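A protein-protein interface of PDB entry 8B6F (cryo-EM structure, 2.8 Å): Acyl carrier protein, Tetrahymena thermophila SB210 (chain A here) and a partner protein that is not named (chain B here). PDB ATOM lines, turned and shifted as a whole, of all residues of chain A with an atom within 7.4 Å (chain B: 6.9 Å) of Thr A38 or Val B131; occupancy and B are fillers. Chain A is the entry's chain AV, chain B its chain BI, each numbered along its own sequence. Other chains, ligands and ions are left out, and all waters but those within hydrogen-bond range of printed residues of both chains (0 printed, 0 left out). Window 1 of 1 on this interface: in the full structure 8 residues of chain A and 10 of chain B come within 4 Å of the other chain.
Of the printed residues of chain B, Glu A37 touches Val B131 and Arg B132.
Of the printed residues of chain B, Thr A38 touches Val B131 (3.7 Å).
Of the printed residues of chain B, Phe A53 touches Thr B137.
Val B131 touches three residues of chain A.
Of the printed residues of chain A, Arg B132 touches Arg A35 and Glu A37.
The nearest residue of chain B that does not touch Thr A38 is Glu B127 (6.3 Å).
The nearest printed residue of chain B that does not touch Phe A53 is Val B131 (4.9 Å).
Arg A35 touches Arg B128.
CD of Arg A35 touches CG2 of Val B131, 3.6 Å away.
NH1 of Arg A35 touches NH2 of Arg B132, at 3.6 Å.
Glu A37 touches Val B131 (CB to O, 3.8 Å).
CG2 of Thr A38 touches CB of Val B131, at 3.7 Å.
Phe A53 touches Thr B137.
Hydrophobic or aromatic side chains of chain A within 4 Å of the printed part of chain B: Phe A53.
Along chain A the printed residues that touch a printed residue of chain B span positions 33 to 53.
Printed residues of chain B that touch a printed residue of chain A: Glu B127, Arg B128, Val B131, Arg B132 and Thr B137.
Among the printed residues, Asp or Glu carboxylates within 4 Å of a Lys or Arg side-chain nitrogen of the other chain: Arg A33 with Glu B127 (2.4 Å) and Glu A37 with Arg B132 (3.7 Å).
The side-chain carboxylate of Glu B127 lies within salt-bridge range of the guanidinium group of Arg A33 (3.9 Å).
OE2 of Glu A37 is in salt-bridge range of NE of Arg B132 (3.7 Å).
The backbone carbonyl oxygen of Phe A53 sits close to the side-chain amide oxygen of Asn A51, at 2.9 Å.
O of Glu A37 lies within hydrogen-bond range of NZ of Lys A52 (3.1 Å).
The side-chain hydroxyl (OG1) of Thr A38 sits at hydrogen-bond distance from the backbone carbonyl oxygen (O) of Arg A35 (2.6 Å).
The side-chain amide nitrogen (NE2) of Gln B108 sits at hydrogen-bond distance from the side-chain hydroxyl (OG1) of Thr B137, 3.5 Å away.
The side-chain hydroxyl (OG1) of Thr B137 is in hydrogen-bond range of the backbone carbonyl oxygen (O) of Tyr B135, at 3.5 Å.
The backbone carbonyl oxygen (O) of Leu B130 sits at hydrogen-bond distance from the side-chain hydroxyl (OG1) of Thr B137 (3.4 Å).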
ATOM      1  N   ARG A  33     -13.763 -31.093  -0.054  1.00  0.00           N
ATOM      2  CA  ARG A  33     -14.089 -29.917   0.739  1.00  0.00           C
ATOM      3  C   ARG A  33     -15.484 -29.985   1.346  1.00  0.00           C
ATOM      4  O   ARG A  33     -15.919 -29.016   1.975  1.00  0.00           O
ATOM      5  CB  ARG A  33     -13.967 -28.658  -0.125  1.00  0.00           C
ATOM      6  CG  ARG A  33     -12.680 -28.586  -0.940  1.00  0.00           C
ATOM      7  CD  ARG A  33     -11.453 -28.528  -0.047  1.00  0.00           C
ATOM      8  NE  ARG A  33     -10.220 -28.454  -0.822  1.00  0.00           N
ATOM      9  CZ  ARG A  33      -9.693 -27.334  -1.296  1.00  0.00           C
ATOM     10  NH1 ARG A  33     -10.275 -26.163  -1.109  1.00  0.00           N
ATOM     11  NH2 ARG A  33      -8.552 -27.392  -1.977  1.00  0.00           N
ATOM     12  N   SER A  34     -16.187 -31.100   1.172  1.00  0.00           N
ATOM     13  CA  SER A  34     -17.566 -31.210   1.626  1.00  0.00           C
ATOM     14  C   SER A  34     -17.639 -31.310   3.144  1.00  0.00           C
ATOM     15  O   SER A  34     -16.785 -31.922   3.787  1.00  0.00           O
ATOM     16  CB  SER A  34     -18.231 -32.429   0.992  1.00  0.00           C
ATOM     17  OG  SER A  34     -17.548 -33.620   1.344  1.00  0.00           O
ATOM     18  N   ARG A  35     -18.671 -30.696   3.712  1.00  0.00           N
ATOM     19  CA  ARG A  35     -18.961 -30.797   5.135  1.00  0.00           C
ATOM     20  C   ARG A  35     -20.434 -30.465   5.331  1.00  0.00           C
ATOM     21  O   ARG A  35     -21.159 -30.181   4.374  1.00  0.00           O
ATOM     22  CB  ARG A  35     -18.051 -29.878   5.955  1.00  0.00           C
ATOM     23  CG  ARG A  35     -18.098 -28.419   5.537  1.00  0.00           C
ATOM     24  CD  ARG A  35     -17.133 -27.572   6.352  1.00  0.00           C
ATOM     25  NE  ARG A  35     -15.750 -28.013   6.204  1.00  0.00           N
ATOM     26  CZ  ARG A  35     -15.087 -28.759   7.080  1.00  0.00           C
ATOM     27  NH1 ARG A  35     -15.644 -29.166   8.208  1.00  0.00           N
ATOM     28  NH2 ARG A  35     -13.829 -29.101   6.819  1.00  0.00           N
ATOM     29  N   VAL A  36     -20.880 -30.510   6.588  1.00  0.00           N
ATOM     30  CA  VAL A  36     -22.293 -30.272   6.880  1.00  0.00           C
ATOM     31  C   VAL A  36     -22.698 -28.859   6.482  1.00  0.00           C
ATOM     32  O   VAL A  36     -23.825 -28.627   6.029  1.00  0.00           O
ATOM     33  CB  VAL A  36     -22.589 -30.548   8.366  1.00  0.00           C
ATOM     34  CG1 VAL A  36     -22.398 -32.017   8.673  1.00  0.00           C
ATOM     35  CG2 VAL A  36     -21.717 -29.686   9.269  1.00  0.00           C
ATOM     36  N   GLU A  37     -21.795 -27.891   6.647  1.00  0.00           N
ATOM     37  CA  GLU A  37     -22.125 -26.514   6.304  1.00  0.00           C
ATOM     38  C   GLU A  37     -22.343 -26.312   4.811  1.00  0.00           C
ATOM     39  O   GLU A  37     -22.907 -25.285   4.420  1.00  0.00           O
ATOM     40  CB  GLU A  37     -21.022 -25.565   6.780  1.00  0.00           C
ATOM     41  CG  GLU A  37     -20.872 -25.470   8.289  1.00  0.00           C
ATOM     42  CD  GLU A  37     -20.060 -26.607   8.870  1.00  0.00           C
ATOM     43  OE1 GLU A  37     -19.781 -27.578   8.138  1.00  0.00           O
ATOM     44  OE2 GLU A  37     -19.690 -26.526  10.059  1.00  0.00           O
ATOM     45  N   THR A  38     -21.920 -27.255   3.972  1.00  0.00           N
ATOM     46  CA  THR A  38     -21.984 -27.094   2.526  1.00  0.00           C
ATOM     47  C   THR A  38     -23.194 -27.780   1.907  1.00  0.00           C
ATOM     48  O   THR A  38     -23.282 -27.860   0.678  1.00  0.00           O
ATOM     49  CB  THR A  38     -20.706 -27.624   1.874  1.00  0.00           C
ATOM     50  OG1 THR A  38     -20.549 -29.014   2.179  1.00  0.00           O
ATOM     51  CG2 THR A  38     -19.495 -26.858   2.380  1.00  0.00           C
ATOM     52  N   ASN A  39     -24.122 -28.276   2.719  1.00  0.00           N
ATOM     53  CA  ASN A  39     -25.309 -28.923   2.179  1.00  0.00           C
ATOM     54  C   ASN A  39     -26.105 -27.936   1.335  1.00  0.00           C
ATOM     55  O   ASN A  39     -26.348 -26.801   1.751  1.00  0.00           O
ATOM     56  CB  ASN A  39     -26.170 -29.465   3.318  1.00  0.00           C
ATOM     57  CG  ASN A  39     -27.371 -30.238   2.822  1.00  0.00           C
ATOM     58  OD1 ASN A  39     -27.377 -30.746   1.702  1.00  0.00           O
ATOM     59  ND2 ASN A  39     -28.401 -30.325   3.654  1.00  0.00           N
ATOM     60  N   SER A  40     -26.513 -28.376   0.142  1.00  0.00           N
ATOM     61  CA  SER A  40     -27.229 -27.528  -0.804  1.00  0.00           C
ATOM     62  C   SER A  40     -28.593 -28.101  -1.176  1.00  0.00           C
ATOM     63  O   SER A  40     -29.161 -27.719  -2.202  1.00  0.00           O
ATOM     64  CB  SER A  40     -26.389 -27.310  -2.064  1.00  0.00           C
ATOM     65  OG  SER A  40     -26.122 -28.539  -2.717  1.00  0.00           O
ATOM     66  N   ALA A  41     -29.131 -29.005  -0.363  1.00  0.00           N
ATOM     67  CA  ALA A  41     -30.413 -29.626  -0.664  1.00  0.00           C
ATOM     68  C   ALA A  41     -31.552 -28.715  -0.224  1.00  0.00           C
ATOM     69  O   ALA A  41     -31.579 -28.247   0.918  1.00  0.00           O
ATOM     70  CB  ALA A  41     -30.522 -30.982   0.031  1.00  0.00           C
ATOM     71  N   GLU A  50     -26.189 -26.601  -7.937  1.00  0.00           N
ATOM     72  CA  GLU A  50     -24.769 -26.929  -7.974  1.00  0.00           C
ATOM     73  C   GLU A  50     -24.103 -26.677  -6.626  1.00  0.00           C
ATOM     74  O   GLU A  50     -23.298 -27.492  -6.162  1.00  0.00           O
ATOM     75  CB  GLU A  50     -24.074 -26.122  -9.069  1.00  0.00           C
ATOM     76  CG  GLU A  50     -24.599 -26.402 -10.469  1.00  0.00           C
ATOM     77  CD  GLU A  50     -23.864 -25.612 -11.535  1.00  0.00           C
ATOM     78  OE1 GLU A  50     -22.903 -24.894 -11.189  1.00  0.00           O
ATOM     79  OE2 GLU A  50     -24.249 -25.707 -12.721  1.00  0.00           O
ATOM     80  N   ASN A  51     -24.426 -25.558  -5.981  1.00  0.00           N
ATOM     81  CA  ASN A  51     -23.759 -25.178  -4.745  1.00  0.00           C
ATOM     82  C   ASN A  51     -24.724 -24.402  -3.862  1.00  0.00           C
ATOM     83  O   ASN A  51     -25.767 -23.922  -4.313  1.00  0.00           O
ATOM     84  CB  ASN A  51     -22.500 -24.348  -5.018  1.00  0.00           C
ATOM     85  CG  ASN A  51     -22.778 -23.129  -5.872  1.00  0.00           C
ATOM     86  OD1 ASN A  51     -23.922 -22.700  -6.012  1.00  0.00           O
ATOM     87  ND2 ASN A  51     -21.727 -22.561  -6.452  1.00  0.00           N
ATOM     88  N   LYS A  52     -24.356 -24.290  -2.584  1.00  0.00           N
ATOM     89  CA  LYS A  52     -25.167 -23.557  -1.621  1.00  0.00           C
ATOM     90  C   LYS A  52     -25.250 -22.072  -1.947  1.00  0.00           C
ATOM     91  O   LYS A  52     -26.173 -21.398  -1.478  1.00  0.00           O
ATOM     92  CB  LYS A  52     -24.594 -23.756  -0.217  1.00  0.00           C
ATOM     93  CG  LYS A  52     -25.368 -23.071   0.895  1.00  0.00           C
ATOM     94  CD  LYS A  52     -24.712 -23.332   2.240  1.00  0.00           C
ATOM     95  CE  LYS A  52     -25.466 -22.657   3.369  1.00  0.00           C
ATOM     96  NZ  LYS A  52     -24.798 -22.874   4.683  1.00  0.00           N
ATOM     97  N   PHE A  53     -24.314 -21.551  -2.734  1.00  0.00           N
ATOM     98  CA  PHE A  53     -24.301 -20.129  -3.058  1.00  0.00           C
ATOM     99  C   PHE A  53     -25.422 -19.821  -4.042  1.00  0.00           C
ATOM    100  O   PHE A  53     -25.448 -20.361  -5.152  1.00  0.00           O
ATOM    101  CB  PHE A  53     -22.950 -19.729  -3.648  1.00  0.00           C
ATOM    102  CG  PHE A  53     -21.774 -20.303  -2.915  1.00  0.00           C
ATOM    103  CD1 PHE A  53     -21.802 -20.457  -1.538  1.00  0.00           C
ATOM    104  CD2 PHE A  53     -20.642 -20.698  -3.606  1.00  0.00           C
ATOM    105  CE1 PHE A  53     -20.722 -20.990  -0.865  1.00  0.00           C
ATOM    106  CE2 PHE A  53     -19.559 -21.231  -2.939  1.00  0.00           C
ATOM    107  CZ  PHE A  53     -19.598 -21.377  -1.568  1.00  0.00           C
ATOM    108  N   SER B 105     -13.597 -16.200   9.853  1.00  0.00           N
ATOM    109  CA  SER B 105     -14.077 -15.872   8.517  1.00  0.00           C
ATOM    110  C   SER B 105     -14.724 -14.496   8.535  1.00  0.00           C
ATOM    111  O   SER B 105     -15.826 -14.293   8.025  1.00  0.00           O
ATOM    112  CB  SER B 105     -15.046 -16.937   8.014  1.00  0.00           C
ATOM    113  OG  SER B 105     -16.095 -17.153   8.939  1.00  0.00           O
ATOM    114  N   GLN B 108     -14.078 -11.606   4.710  1.00  0.00           N
ATOM    115  CA  GLN B 108     -14.436 -12.049   3.370  1.00  0.00           C
ATOM    116  C   GLN B 108     -14.592 -10.867   2.423  1.00  0.00           C
ATOM    117  O   GLN B 108     -15.150  -9.828   2.783  1.00  0.00           O
ATOM    118  CB  GLN B 108     -15.734 -12.850   3.404  1.00  0.00           C
ATOM    119  CG  GLN B 108     -15.704 -14.038   4.339  1.00  0.00           C
ATOM    120  CD  GLN B 108     -17.038 -14.744   4.413  1.00  0.00           C
ATOM    121  OE1 GLN B 108     -17.584 -14.945   5.495  1.00  0.00           O
ATOM    122  NE2 GLN B 108     -17.573 -15.125   3.258  1.00  0.00           N
ATOM    123  N   GLU B 126      -8.794 -22.302   4.011  1.00  0.00           N
ATOM    124  CA  GLU B 126      -9.535 -21.095   3.657  1.00  0.00           C
ATOM    125  C   GLU B 126     -10.952 -21.433   3.215  1.00  0.00           C
ATOM    126  O   GLU B 126     -11.910 -20.755   3.600  1.00  0.00           O
ATOM    127  CB  GLU B 126      -8.797 -20.325   2.562  1.00  0.00           C
ATOM    128  CG  GLU B 126      -9.533 -19.083   2.074  1.00  0.00           C
ATOM    129  CD  GLU B 126      -8.730 -18.290   1.061  1.00  0.00           C
ATOM    130  OE1 GLU B 126      -7.557 -18.642   0.827  1.00  0.00           O
ATOM    131  OE2 GLU B 126      -9.271 -17.316   0.498  1.00  0.00           O
ATOM    132  N   GLU B 127     -11.105 -22.483   2.405  1.00  0.00           N
ATOM    133  CA  GLU B 127     -12.435 -22.892   1.972  1.00  0.00           C
ATOM    134  C   GLU B 127     -13.276 -23.361   3.151  1.00  0.00           C
ATOM    135  O   GLU B 127     -14.475 -23.072   3.218  1.00  0.00           O
ATOM    136  CB  GLU B 127     -12.333 -23.988   0.913  1.00  0.00           C
ATOM    137  CG  GLU B 127     -13.685 -24.422   0.371  1.00  0.00           C
ATOM    138  CD  GLU B 127     -13.573 -25.217  -0.912  1.00  0.00           C
ATOM    139  OE1 GLU B 127     -12.451 -25.330  -1.448  1.00  0.00           O
ATOM    140  OE2 GLU B 127     -14.607 -25.727  -1.390  1.00  0.00           O
ATOM    141  N   ARG B 128     -12.667 -24.086   4.090  1.00  0.00           N
ATOM    142  CA  ARG B 128     -13.389 -24.500   5.289  1.00  0.00           C
ATOM    143  C   ARG B 128     -13.946 -23.291   6.030  1.00  0.00           C
ATOM    144  O   ARG B 128     -15.122 -23.269   6.411  1.00  0.00           O
ATOM    145  CB  ARG B 128     -12.465 -25.308   6.199  1.00  0.00           C
ATOM    146  CG  ARG B 128     -13.106 -25.745   7.508  1.00  0.00           C
ATOM    147  CD  ARG B 128     -12.075 -26.302   8.468  1.00  0.00           C
ATOM    148  NE  ARG B 128     -11.153 -25.271   8.924  1.00  0.00           N
ATOM    149  CZ  ARG B 128     -10.152 -25.480   9.768  1.00  0.00           C
ATOM    150  NH1 ARG B 128      -9.909 -26.679  10.270  1.00  0.00           N
ATOM    151  NH2 ARG B 128      -9.375 -24.459  10.118  1.00  0.00           N
ATOM    152  N   ASN B 129     -13.109 -22.284   6.267  1.00  0.00           N
ATOM    153  CA  ASN B 129     -13.568 -21.098   6.983  1.00  0.00           C
ATOM    154  C   ASN B 129     -14.657 -20.369   6.205  1.00  0.00           C
ATOM    155  O   ASN B 129     -15.651 -19.923   6.786  1.00  0.00           O
ATOM    156  CB  ASN B 129     -12.389 -20.171   7.263  1.00  0.00           C
ATOM    157  CG  ASN B 129     -11.452 -20.730   8.313  1.00  0.00           C
ATOM    158  OD1 ASN B 129     -11.491 -20.327   9.473  1.00  0.00           O
ATOM    159  ND2 ASN B 129     -10.611 -21.675   7.911  1.00  0.00           N
ATOM    160  N   LEU B 130     -14.483 -20.229   4.892  1.00  0.00           N
ATOM    161  CA  LEU B 130     -15.476 -19.525   4.086  1.00  0.00           C
ATOM    162  C   LEU B 130     -16.833 -20.214   4.157  1.00  0.00           C
ATOM    163  O   LEU B 130     -17.862 -19.561   4.356  1.00  0.00           O
ATOM    164  CB  LEU B 130     -15.001 -19.424   2.636  1.00  0.00           C
ATOM    165  CG  LEU B 130     -13.828 -18.480   2.363  1.00  0.00           C
ATOM    166  CD1 LEU B 130     -13.375 -18.596   0.921  1.00  0.00           C
ATOM    167  CD2 LEU B 130     -14.200 -17.045   2.684  1.00  0.00           C
ATOM    168  N   VAL B 131     -16.857 -21.539   4.003  1.00  0.00           N
ATOM    169  CA  VAL B 131     -18.128 -22.257   4.055  1.00  0.00           C
ATOM    170  C   VAL B 131     -18.724 -22.198   5.454  1.00  0.00           C
ATOM    171  O   VAL B 131     -19.949 -22.141   5.612  1.00  0.00           O
ATOM    172  CB  VAL B 131     -17.957 -23.712   3.575  1.00  0.00           C
ATOM    173  CG1 VAL B 131     -17.460 -23.742   2.140  1.00  0.00           C
ATOM    174  CG2 VAL B 131     -17.018 -24.481   4.482  1.00  0.00           C
ATOM    175  N   ARG B 132     -17.883 -22.215   6.489  1.00  0.00           N
ATOM    176  CA  ARG B 132     -18.372 -22.093   7.855  1.00  0.00           C
ATOM    177  C   ARG B 132     -18.840 -20.685   8.192  1.00  0.00           C
ATOM    178  O   ARG B 132     -19.433 -20.489   9.258  1.00  0.00           O
ATOM    179  CB  ARG B 132     -17.282 -22.514   8.842  1.00  0.00           C
ATOM    180  CG  ARG B 132     -17.098 -24.016   8.951  1.00  0.00           C
ATOM    181  CD  ARG B 132     -16.035 -24.371   9.975  1.00  0.00           C
ATOM    182  NE  ARG B 132     -16.093 -25.780  10.343  1.00  0.00           N
ATOM    183  CZ  ARG B 132     -15.267 -26.368  11.197  1.00  0.00           C
ATOM    184  NH1 ARG B 132     -14.294 -25.698  11.791  1.00  0.00           N
ATOM    185  NH2 ARG B 132     -15.425 -27.660  11.465  1.00  0.00           N
ATOM    186  N   SER B 133     -18.588 -19.706   7.325  1.00  0.00           N
ATOM    187  CA  SER B 133     -19.069 -18.353   7.563  1.00  0.00           C
ATOM    188  C   SER B 133     -20.574 -18.348   7.790  1.00  0.00           C
ATOM    189  O   SER B 133     -21.326 -19.049   7.108  1.00  0.00           O
ATOM    190  CB  SER B 133     -18.719 -17.453   6.376  1.00  0.00           C
ATOM    191  OG  SER B 133     -19.209 -16.139   6.577  1.00  0.00           O
ATOM    192  N   SER B 134     -21.011 -17.549   8.765  1.00  0.00           N
ATOM    193  CA  SER B 134     -22.423 -17.514   9.129  1.00  0.00           C
ATOM    194  C   SER B 134     -23.263 -16.744   8.116  1.00  0.00           C
ATOM    195  O   SER B 134     -24.443 -17.064   7.929  1.00  0.00           O
ATOM    196  CB  SER B 134     -22.585 -16.907  10.522  1.00  0.00           C
ATOM    197  OG  SER B 134     -22.001 -15.620  10.590  1.00  0.00           O
ATOM    198  N   TYR B 135     -22.695 -15.732   7.472  1.00  0.00           N
ATOM    199  CA  TYR B 135     -23.411 -14.973   6.459  1.00  0.00           C
ATOM    200  C   TYR B 135     -23.278 -15.638   5.097  1.00  0.00           C
ATOM    201  O   TYR B 135     -22.421 -16.502   4.894  1.00  0.00           O
ATOM    202  CB  TYR B 135     -22.874 -13.544   6.398  1.00  0.00           C
ATOM    203  CG  TYR B 135     -23.302 -12.654   7.548  1.00  0.00           C
ATOM    204  CD1 TYR B 135     -24.095 -13.141   8.581  1.00  0.00           C
ATOM    205  CD2 TYR B 135     -22.921 -11.321   7.592  1.00  0.00           C
ATOM    206  CE1 TYR B 135     -24.487 -12.328   9.624  1.00  0.00           C
ATOM    207  CE2 TYR B 135     -23.308 -10.501   8.633  1.00  0.00           C
ATOM    208  CZ  TYR B 135     -24.090 -11.011   9.646  1.00  0.00           C
ATOM    209  OH  TYR B 135     -24.480 -10.198  10.684  1.00  0.00           O
ATOM    210  N   THR B 137     -22.258 -16.589   1.337  1.00  0.00           N
ATOM    211  CA  THR B 137     -20.962 -16.554   0.678  1.00  0.00           C
ATOM    212  C   THR B 137     -21.156 -16.710  -0.825  1.00  0.00           C
ATOM    213  O   THR B 137     -22.182 -17.211  -1.290  1.00  0.00           O
ATOM    214  CB  THR B 137     -20.040 -17.662   1.217  1.00  0.00           C
ATOM    215  OG1 THR B 137     -19.984 -17.586   2.646  1.00  0.00           O
ATOM    216  CG2 THR B 137     -18.627 -17.531   0.663  1.00  0.00           C
